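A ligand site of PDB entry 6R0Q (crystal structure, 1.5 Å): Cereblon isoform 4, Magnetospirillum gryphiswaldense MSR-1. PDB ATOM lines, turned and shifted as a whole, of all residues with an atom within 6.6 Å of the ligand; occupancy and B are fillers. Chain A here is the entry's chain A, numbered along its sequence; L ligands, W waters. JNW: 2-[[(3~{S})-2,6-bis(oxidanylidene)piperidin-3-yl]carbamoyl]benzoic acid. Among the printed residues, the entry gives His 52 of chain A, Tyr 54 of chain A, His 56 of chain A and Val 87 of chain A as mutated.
A ring nitrogen (NE2) of His 56 sits at hydrogen-bond distance from an oxygen (OAS) of the ligand, at 2.7 Å.
The side-chain hydroxyl (OH) of Tyr 101 lies within hydrogen-bond range of an oxygen (OE1) of the ligand, at 2.7 Å.
The backbone carbonyl oxygen (O) of Phe 77 lies within hydrogen-bond range of a nitrogen (NE2) of the ligand (2.8 Å).
The side-chain amide nitrogen (ND2) of Asn 50 sits at hydrogen-bond distance from an oxygen (OAS) of the ligand (2.9 Å).
The backbone NH (N) of Trp 79 is in hydrogen-bond range of an oxygen (OE1) of the ligand (3.0 Å).
N of His 52 is in hydrogen-bond range of OD1 of Asn 50, 2.9 Å away.
The side-chain amide oxygen of Asn 50 sits at hydrogen-bond distance from the backbone NH of Tyr 54, at 3.0 Å.
The indole nitrogen (NE1) of Trp 79 sits at hydrogen-bond distance from the backbone carbonyl oxygen (O) of Phe 49, at 2.9 Å.
NE1 of Trp 99 lies within hydrogen-bond range of NE2 of His 96 (3.5 Å).
The side-chain hydroxyl of Ser 78 lies within hydrogen-bond range of the backbone carbonyl oxygen of Phe 80, 2.9 Å away.
The backbone carbonyl oxygen of His 96 lies within hydrogen-bond range of the guanidinium group of Arg 117 (2.9 Å).
NE1 of Trp 85 sits at hydrogen-bond distance from O of Glu 76 (2.9 Å).
CD of Pro 51 touches O of the ligand, at 3.4 Å.
CD2 of His 52 touches CAO of the ligand (3.8 Å).
Ser 78 touches the ligand (CA to OE1, 3.4 Å).
Trp 85 touches the ligand.
His 96 touches the ligand.
Trp 99 touches the ligand (CZ2 to OAT, 3.4 Å).
Of the 19 residues printed, 11 come within 4 Å of the ligand.
The nearest printed residue that does not touch the ligand is Phe 49 (4.4 Å).
Water W1 bridges an oxygen (OAT) of the ligand (2.9 Å) and the indole nitrogen (NE1) of Trp 99 (2.9 Å).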
ATOM      1  N   PHE A  49     -23.988 -14.810 -18.868  1.00  0.00           N
ATOM      2  CA  PHE A  49     -24.554 -14.755 -17.516  1.00  0.00           C
ATOM      3  C   PHE A  49     -25.068 -16.075 -17.123  1.00  0.00           C
ATOM      4  O   PHE A  49     -25.491 -16.912 -17.960  1.00  0.00           O
ATOM      5  CB  PHE A  49     -25.645 -13.659 -17.448  1.00  0.00           C
ATOM      6  CG  PHE A  49     -26.714 -13.684 -18.458  1.00  0.00           C
ATOM      7  CD1 PHE A  49     -27.850 -14.500 -18.313  1.00  0.00           C
ATOM      8  CD2 PHE A  49     -26.521 -12.950 -19.618  1.00  0.00           C
ATOM      9  CE1 PHE A  49     -28.793 -14.531 -19.312  1.00  0.00           C
ATOM     10  CE2 PHE A  49     -27.504 -12.971 -20.533  1.00  0.00           C
ATOM     11  CZ  PHE A  49     -28.543 -13.765 -20.468  1.00  0.00           C
ATOM     12  N   ASN A  50     -25.042 -16.369 -15.805  1.00  0.00           N
ATOM     13  CA  ASN A  50     -25.538 -17.603 -15.325  1.00  0.00           C
ATOM     14  C   ASN A  50     -27.056 -17.555 -15.247  1.00  0.00           C
ATOM     15  O   ASN A  50     -27.682 -16.554 -15.530  1.00  0.00           O
ATOM     16  CB  ASN A  50     -24.810 -17.936 -13.999  1.00  0.00           C
ATOM     17  CG  ASN A  50     -25.173 -17.036 -12.858  1.00  0.00           C
ATOM     18  OD1 ASN A  50     -26.213 -16.314 -12.809  1.00  0.00           O
ATOM     19  ND2 ASN A  50     -24.275 -17.010 -11.803  1.00  0.00           N
ATOM     20  N   PRO A  51     -27.685 -18.650 -14.832  1.00  0.00           N
ATOM     21  CA  PRO A  51     -29.194 -18.642 -14.836  1.00  0.00           C
ATOM     22  C   PRO A  51     -29.769 -17.871 -13.733  1.00  0.00           C
ATOM     23  O   PRO A  51     -31.010 -17.859 -13.560  1.00  0.00           O
ATOM     24  CB  PRO A  51     -29.497 -20.175 -14.649  1.00  0.00           C
ATOM     25  CG  PRO A  51     -28.330 -20.843 -15.043  1.00  0.00           C
ATOM     26  CD  PRO A  51     -27.099 -20.017 -14.654  1.00  0.00           C
ATOM     27  N   HIS A  52     -28.962 -17.223 -12.897  1.00  0.00           N
ATOM     28  CA  HIS A  52     -29.426 -16.241 -11.917  1.00  0.00           C
ATOM     29  C   HIS A  52     -29.212 -14.850 -12.320  1.00  0.00           C
ATOM     30  O   HIS A  52     -29.333 -13.904 -11.542  1.00  0.00           O
ATOM     31  CB  HIS A  52     -28.808 -16.528 -10.562  1.00  0.00           C
ATOM     32  CG  HIS A  52     -28.998 -17.912 -10.133  1.00  0.00           C
ATOM     33  ND1 HIS A  52     -30.281 -18.370  -9.867  1.00  0.00           N
ATOM     34  CD2 HIS A  52     -28.193 -18.980 -10.019  1.00  0.00           C
ATOM     35  CE1 HIS A  52     -30.203 -19.670  -9.554  1.00  0.00           C
ATOM     36  NE2 HIS A  52     -28.961 -20.062  -9.674  1.00  0.00           N
ATOM     37  N   TYR A  54     -26.283 -13.324 -13.159  1.00  0.00           N
ATOM     38  CA  TYR A  54     -25.010 -12.749 -12.844  1.00  0.00           C
ATOM     39  C   TYR A  54     -24.091 -12.795 -14.089  1.00  0.00           C
ATOM     40  O   TYR A  54     -23.899 -13.925 -14.630  1.00  0.00           O
ATOM     41  CB  TYR A  54     -24.354 -13.501 -11.740  1.00  0.00           C
ATOM     42  CG  TYR A  54     -23.144 -12.764 -11.130  1.00  0.00           C
ATOM     43  CD1 TYR A  54     -23.278 -11.829 -10.109  1.00  0.00           C
ATOM     44  CD2 TYR A  54     -21.933 -13.053 -11.603  1.00  0.00           C
ATOM     45  CE1 TYR A  54     -22.131 -11.152  -9.630  1.00  0.00           C
ATOM     46  CE2 TYR A  54     -20.789 -12.361 -11.195  1.00  0.00           C
ATOM     47  CZ  TYR A  54     -20.990 -11.440 -10.190  1.00  0.00           C
ATOM     48  OH  TYR A  54     -19.746 -10.867  -9.755  1.00  0.00           O
ATOM     49  N   HIS A  56     -20.743 -12.876 -16.295  1.00  0.00           N
ATOM     50  CA  HIS A  56     -19.361 -13.211 -16.311  1.00  0.00           C
ATOM     51  C   HIS A  56     -18.782 -12.861 -17.701  1.00  0.00           C
ATOM     52  O   HIS A  56     -19.356 -13.205 -18.703  1.00  0.00           O
ATOM     53  CB  HIS A  56     -19.107 -14.714 -16.079  1.00  0.00           C
ATOM     54  CG  HIS A  56     -19.486 -15.215 -14.749  1.00  0.00           C
ATOM     55  ND1 HIS A  56     -18.917 -14.782 -13.584  1.00  0.00           N
ATOM     56  CD2 HIS A  56     -20.315 -16.237 -14.431  1.00  0.00           C
ATOM     57  CE1 HIS A  56     -19.465 -15.479 -12.592  1.00  0.00           C
ATOM     58  NE2 HIS A  56     -20.313 -16.360 -13.049  1.00  0.00           N
ATOM     59  N   GLU A  76     -26.654 -28.970 -18.944  1.00  0.00           N
ATOM     60  CA  GLU A  76     -27.704 -27.964 -18.721  1.00  0.00           C
ATOM     61  C   GLU A  76     -27.061 -26.568 -18.757  1.00  0.00           C
ATOM     62  O   GLU A  76     -26.057 -26.342 -18.145  1.00  0.00           O
ATOM     63  CB  GLU A  76     -28.272 -28.217 -17.292  1.00  0.00           C
ATOM     64  CG  GLU A  76     -29.652 -28.870 -17.013  1.00  0.00           C
ATOM     65  CD  GLU A  76     -30.490 -28.101 -15.890  1.00  0.00           C
ATOM     66  OE1 GLU A  76     -29.883 -27.832 -14.736  1.00  0.00           O
ATOM     67  OE2 GLU A  76     -31.729 -27.752 -16.105  1.00  0.00           O
ATOM     68  N   PHE A  77     -27.699 -25.635 -19.443  1.00  0.00           N
ATOM     69  CA  PHE A  77     -27.301 -24.235 -19.474  1.00  0.00           C
ATOM     70  C   PHE A  77     -25.966 -23.920 -20.101  1.00  0.00           C
ATOM     71  O   PHE A  77     -25.363 -22.864 -19.837  1.00  0.00           O
ATOM     72  CB  PHE A  77     -27.378 -23.607 -18.109  1.00  0.00           C
ATOM     73  CG  PHE A  77     -28.724 -23.669 -17.473  1.00  0.00           C
ATOM     74  CD1 PHE A  77     -29.763 -22.908 -17.951  1.00  0.00           C
ATOM     75  CD2 PHE A  77     -28.922 -24.431 -16.277  1.00  0.00           C
ATOM     76  CE1 PHE A  77     -31.005 -22.930 -17.336  1.00  0.00           C
ATOM     77  CE2 PHE A  77     -30.248 -24.413 -15.754  1.00  0.00           C
ATOM     78  CZ  PHE A  77     -31.190 -23.648 -16.218  1.00  0.00           C
ATOM     79  N   SER A  78     -25.405 -24.808 -20.917  1.00  0.00           N
ATOM     80  CA  SER A  78     -24.163 -24.495 -21.470  1.00  0.00           C
ATOM     81  C   SER A  78     -24.226 -23.324 -22.370  1.00  0.00           C
ATOM     82  O   SER A  78     -25.111 -23.221 -23.222  1.00  0.00           O
ATOM     83  CB  SER A  78     -23.626 -25.670 -22.382  1.00  0.00           C
ATOM     84  OG  SER A  78     -22.349 -25.353 -22.857  1.00  0.00           O
ATOM     85  N   TRP A  79     -23.271 -22.405 -22.245  1.00  0.00           N
ATOM     86  CA  TRP A  79     -23.088 -21.297 -23.081  1.00  0.00           C
ATOM     87  C   TRP A  79     -22.650 -21.616 -24.499  1.00  0.00           C
ATOM     88  O   TRP A  79     -22.775 -20.801 -25.405  1.00  0.00           O
ATOM     89  CB  TRP A  79     -22.213 -20.200 -22.552  1.00  0.00           C
ATOM     90  CG  TRP A  79     -22.685 -19.619 -21.236  1.00  0.00           C
ATOM     91  CD1 TRP A  79     -23.965 -19.072 -20.943  1.00  0.00           C
ATOM     92  CD2 TRP A  79     -21.938 -19.504 -20.014  1.00  0.00           C
ATOM     93  NE1 TRP A  79     -23.995 -18.626 -19.686  1.00  0.00           N
ATOM     94  CE2 TRP A  79     -22.739 -18.805 -19.102  1.00  0.00           C
ATOM     95  CE3 TRP A  79     -20.635 -19.815 -19.676  1.00  0.00           C
ATOM     96  CZ2 TRP A  79     -22.389 -18.562 -17.816  1.00  0.00           C
ATOM     97  CZ3 TRP A  79     -20.235 -19.458 -18.458  1.00  0.00           C
ATOM     98  CH2 TRP A  79     -21.035 -18.932 -17.503  1.00  0.00           C
ATOM     99  N   PHE A  80     -22.131 -22.817 -24.697  1.00  0.00           N
ATOM    100  CA  PHE A  80     -21.482 -23.277 -25.921  1.00  0.00           C
ATOM    101  C   PHE A  80     -22.120 -24.491 -26.368  1.00  0.00           C
ATOM    102  O   PHE A  80     -22.144 -25.552 -25.746  1.00  0.00           O
ATOM    103  CB  PHE A  80     -19.971 -23.449 -25.641  1.00  0.00           C
ATOM    104  CG  PHE A  80     -19.313 -22.243 -25.247  1.00  0.00           C
ATOM    105  CD1 PHE A  80     -18.974 -21.202 -26.146  1.00  0.00           C
ATOM    106  CD2 PHE A  80     -19.004 -22.002 -23.926  1.00  0.00           C
ATOM    107  CE1 PHE A  80     -18.307 -20.042 -25.648  1.00  0.00           C
ATOM    108  CE2 PHE A  80     -18.410 -20.827 -23.477  1.00  0.00           C
ATOM    109  CZ  PHE A  80     -18.011 -19.872 -24.335  1.00  0.00           C
ATOM    110  N   TRP A  85     -20.166 -29.185 -19.457  1.00  0.00           N
ATOM    111  CA  TRP A  85     -19.183 -28.454 -18.663  1.00  0.00           C
ATOM    112  C   TRP A  85     -19.068 -28.931 -17.247  1.00  0.00           C
ATOM    113  O   TRP A  85     -19.993 -29.494 -16.704  1.00  0.00           O
ATOM    114  CB  TRP A  85     -19.582 -26.911 -18.603  1.00  0.00           C
ATOM    115  CG  TRP A  85     -20.996 -26.640 -18.090  1.00  0.00           C
ATOM    116  CD1 TRP A  85     -22.111 -26.502 -18.844  1.00  0.00           C
ATOM    117  CD2 TRP A  85     -21.427 -26.577 -16.769  1.00  0.00           C
ATOM    118  NE1 TRP A  85     -23.161 -26.392 -18.108  1.00  0.00           N
ATOM    119  CE2 TRP A  85     -22.814 -26.368 -16.759  1.00  0.00           C
ATOM    120  CE3 TRP A  85     -20.775 -26.574 -15.562  1.00  0.00           C
ATOM    121  CZ2 TRP A  85     -23.533 -26.282 -15.600  1.00  0.00           C
ATOM    122  CZ3 TRP A  85     -21.464 -26.475 -14.420  1.00  0.00           C
ATOM    123  CH2 TRP A  85     -22.888 -26.344 -14.390  1.00  0.00           C
ATOM    124  N   THR A  86     -17.889 -28.634 -16.670  1.00  0.00           N
ATOM    125  CA  THR A  86     -17.488 -28.924 -15.321  1.00  0.00           C
ATOM    126  C   THR A  86     -16.799 -27.772 -14.712  1.00  0.00           C
ATOM    127  O   THR A  86     -15.979 -27.162 -15.348  1.00  0.00           O
ATOM    128  CB  THR A  86     -16.542 -30.102 -15.301  1.00  0.00           C
ATOM    129  OG1 THR A  86     -17.131 -31.267 -16.035  1.00  0.00           O
ATOM    130  CG2 THR A  86     -16.325 -30.606 -13.839  1.00  0.00           C
ATOM    131  N   VAL A  87     -17.176 -27.440 -13.476  1.00  0.00           N
ATOM    132  CA  VAL A  87     -16.454 -26.454 -12.701  1.00  0.00           C
ATOM    133  C   VAL A  87     -14.956 -26.710 -12.631  1.00  0.00           C
ATOM    134  O   VAL A  87     -14.554 -27.847 -12.383  1.00  0.00           O
ATOM    135  CB  VAL A  87     -17.007 -26.381 -11.303  1.00  0.00           C
ATOM    136  CG1 VAL A  87     -16.096 -25.621 -10.300  1.00  0.00           C
ATOM    137  CG2 VAL A  87     -18.408 -25.702 -11.280  1.00  0.00           C
ATOM    138  N   HIS A  96     -12.494 -20.350  -7.898  1.00  0.00           N
ATOM    139  CA  HIS A  96     -13.284 -20.796  -9.071  1.00  0.00           C
ATOM    140  C   HIS A  96     -12.950 -20.014 -10.305  1.00  0.00           C
ATOM    141  O   HIS A  96     -13.431 -18.905 -10.480  1.00  0.00           O
ATOM    142  CB  HIS A  96     -14.734 -20.737  -8.736  1.00  0.00           C
ATOM    143  CG  HIS A  96     -15.585 -21.211  -9.875  1.00  0.00           C
ATOM    144  ND1 HIS A  96     -16.953 -20.946  -9.909  1.00  0.00           N
ATOM    145  CD2 HIS A  96     -15.311 -21.977 -10.920  1.00  0.00           C
ATOM    146  CE1 HIS A  96     -17.423 -21.472 -11.070  1.00  0.00           C
ATOM    147  NE2 HIS A  96     -16.450 -22.087 -11.692  1.00  0.00           N
ATOM    148  N   TRP A  99     -14.653 -23.011 -16.105  1.00  0.00           N
ATOM    149  CA  TRP A  99     -15.235 -24.274 -16.465  1.00  0.00           C
ATOM    150  C   TRP A  99     -14.439 -24.945 -17.620  1.00  0.00           C
ATOM    151  O   TRP A  99     -13.941 -24.254 -18.487  1.00  0.00           O
ATOM    152  CB  TRP A  99     -16.732 -24.131 -16.904  1.00  0.00           C
ATOM    153  CG  TRP A  99     -17.585 -23.380 -15.936  1.00  0.00           C
ATOM    154  CD1 TRP A  99     -18.241 -23.840 -14.887  1.00  0.00           C
ATOM    155  CD2 TRP A  99     -17.642 -21.965 -15.832  1.00  0.00           C
ATOM    156  NE1 TRP A  99     -18.773 -22.830 -14.139  1.00  0.00           N
ATOM    157  CE2 TRP A  99     -18.450 -21.638 -14.731  1.00  0.00           C
ATOM    158  CE3 TRP A  99     -17.161 -20.940 -16.651  1.00  0.00           C
ATOM    159  CZ2 TRP A  99     -18.750 -20.314 -14.366  1.00  0.00           C
ATOM    160  CZ3 TRP A  99     -17.446 -19.636 -16.265  1.00  0.00           C
ATOM    161  CH2 TRP A  99     -18.234 -19.342 -15.148  1.00  0.00           C
ATOM    162  N   TYR A 101     -15.005 -27.554 -20.815  1.00  0.00           N
ATOM    163  CA  TYR A 101     -15.999 -27.989 -21.707  1.00  0.00           C
ATOM    164  C   TYR A 101     -15.509 -29.198 -22.472  1.00  0.00           C
ATOM    165  O   TYR A 101     -14.338 -29.186 -22.955  1.00  0.00           O
ATOM    166  CB  TYR A 101     -16.314 -26.850 -22.677  1.00  0.00           C
ATOM    167  CG  TYR A 101     -17.000 -25.667 -22.010  1.00  0.00           C
ATOM    168  CD1 TYR A 101     -16.323 -24.625 -21.433  1.00  0.00           C
ATOM    169  CD2 TYR A 101     -18.396 -25.646 -21.970  1.00  0.00           C
ATOM    170  CE1 TYR A 101     -17.021 -23.588 -20.777  1.00  0.00           C
ATOM    171  CE2 TYR A 101     -19.090 -24.627 -21.343  1.00  0.00           C
ATOM    172  CZ  TYR A 101     -18.403 -23.639 -20.732  1.00  0.00           C
ATOM    173  OH  TYR A 101     -19.022 -22.574 -20.093  1.00  0.00           O
ATOM    174  N   ILE A 114     -12.944 -17.211 -16.310  1.00  0.00           N
ATOM    175  CA  ILE A 114     -13.491 -15.942 -15.959  1.00  0.00           C
ATOM    176  C   ILE A 114     -12.393 -14.890 -15.904  1.00  0.00           C
ATOM    177  O   ILE A 114     -11.481 -14.956 -15.070  1.00  0.00           O
ATOM    178  CB  ILE A 114     -14.246 -15.977 -14.562  1.00  0.00           C
ATOM    179  CG1 ILE A 114     -15.347 -17.008 -14.664  1.00  0.00           C
ATOM    180  CG2 ILE A 114     -14.663 -14.673 -14.144  1.00  0.00           C
ATOM    181  CD1 ILE A 114     -15.860 -17.419 -13.260  1.00  0.00           C
ATOM    182  N   ARG A 117     -11.035 -13.146 -12.767  1.00  0.00           N
ATOM    183  CA  ARG A 117     -10.440 -14.002 -11.787  1.00  0.00           C
ATOM    184  C   ARG A 117      -9.018 -14.439 -12.191  1.00  0.00           C
ATOM    185  O   ARG A 117      -8.371 -15.197 -11.473  1.00  0.00           O
ATOM    186  CB  ARG A 117     -11.296 -15.251 -11.479  1.00  0.00           C
ATOM    187  CG  ARG A 117     -12.603 -14.762 -10.843  1.00  0.00           C
ATOM    188  CD  ARG A 117     -13.458 -15.846 -10.382  1.00  0.00           C
ATOM    189  NE  ARG A 117     -14.792 -15.352  -9.889  1.00  0.00           N
ATOM    190  CZ  ARG A 117     -15.844 -16.049  -9.789  1.00  0.00           C
ATOM    191  NH1 ARG A 117     -15.817 -17.370  -9.819  1.00  0.00           N
ATOM    192  NH2 ARG A 117     -17.048 -15.439  -9.467  1.00  0.00           N
HETATM  193  OAS JNW L   1     -21.653 -18.133 -11.538  1.00  0.00           O
HETATM  194  CAR JNW L   1     -21.767 -19.312 -11.519  1.00  0.00           C
HETATM  195  OAT JNW L   1     -20.636 -19.878 -11.593  1.00  0.00           O
HETATM  196  CAQ JNW L   1     -22.957 -19.998 -11.380  1.00  0.00           C
HETATM  197  CAP JNW L   1     -23.741 -19.911 -10.320  1.00  0.00           C
HETATM  198  CAO JNW L   1     -24.812 -20.659 -10.098  1.00  0.00           C
HETATM  199  CAN JNW L   1     -25.290 -21.435 -10.974  1.00  0.00           C
HETATM  200  CAM JNW L   1     -24.692 -21.519 -12.126  1.00  0.00           C
HETATM  201  CAK JNW L   1     -23.494 -20.887 -12.340  1.00  0.00           C
HETATM  202  CAJ JNW L   1     -22.911 -20.760 -13.594  1.00  0.00           C
HETATM  203  OAL JNW L   1     -22.216 -19.840 -14.077  1.00  0.00           O
HETATM  204  N   JNW L   1     -23.056 -21.687 -14.509  1.00  0.00           N
HETATM  205  CA  JNW L   1     -22.489 -21.799 -15.847  1.00  0.00           C
HETATM  206  CB  JNW L   1     -21.591 -22.933 -16.182  1.00  0.00           C
HETATM  207  CG  JNW L   1     -20.972 -22.937 -17.392  1.00  0.00           C
HETATM  208  CD  JNW L   1     -21.947 -22.716 -18.562  1.00  0.00           C
HETATM  209  OE1 JNW L   1     -21.716 -22.837 -19.704  1.00  0.00           O
HETATM  210  NE2 JNW L   1     -23.135 -22.090 -18.240  1.00  0.00           N
HETATM  211  C   JNW L   1     -23.522 -21.671 -16.929  1.00  0.00           C
HETATM  212  O   JNW L   1     -24.601 -21.061 -16.737  1.00  0.00           O
HETATM  213  O   HOH W   1     -20.318 -22.716 -11.716  1.00  0.00           O
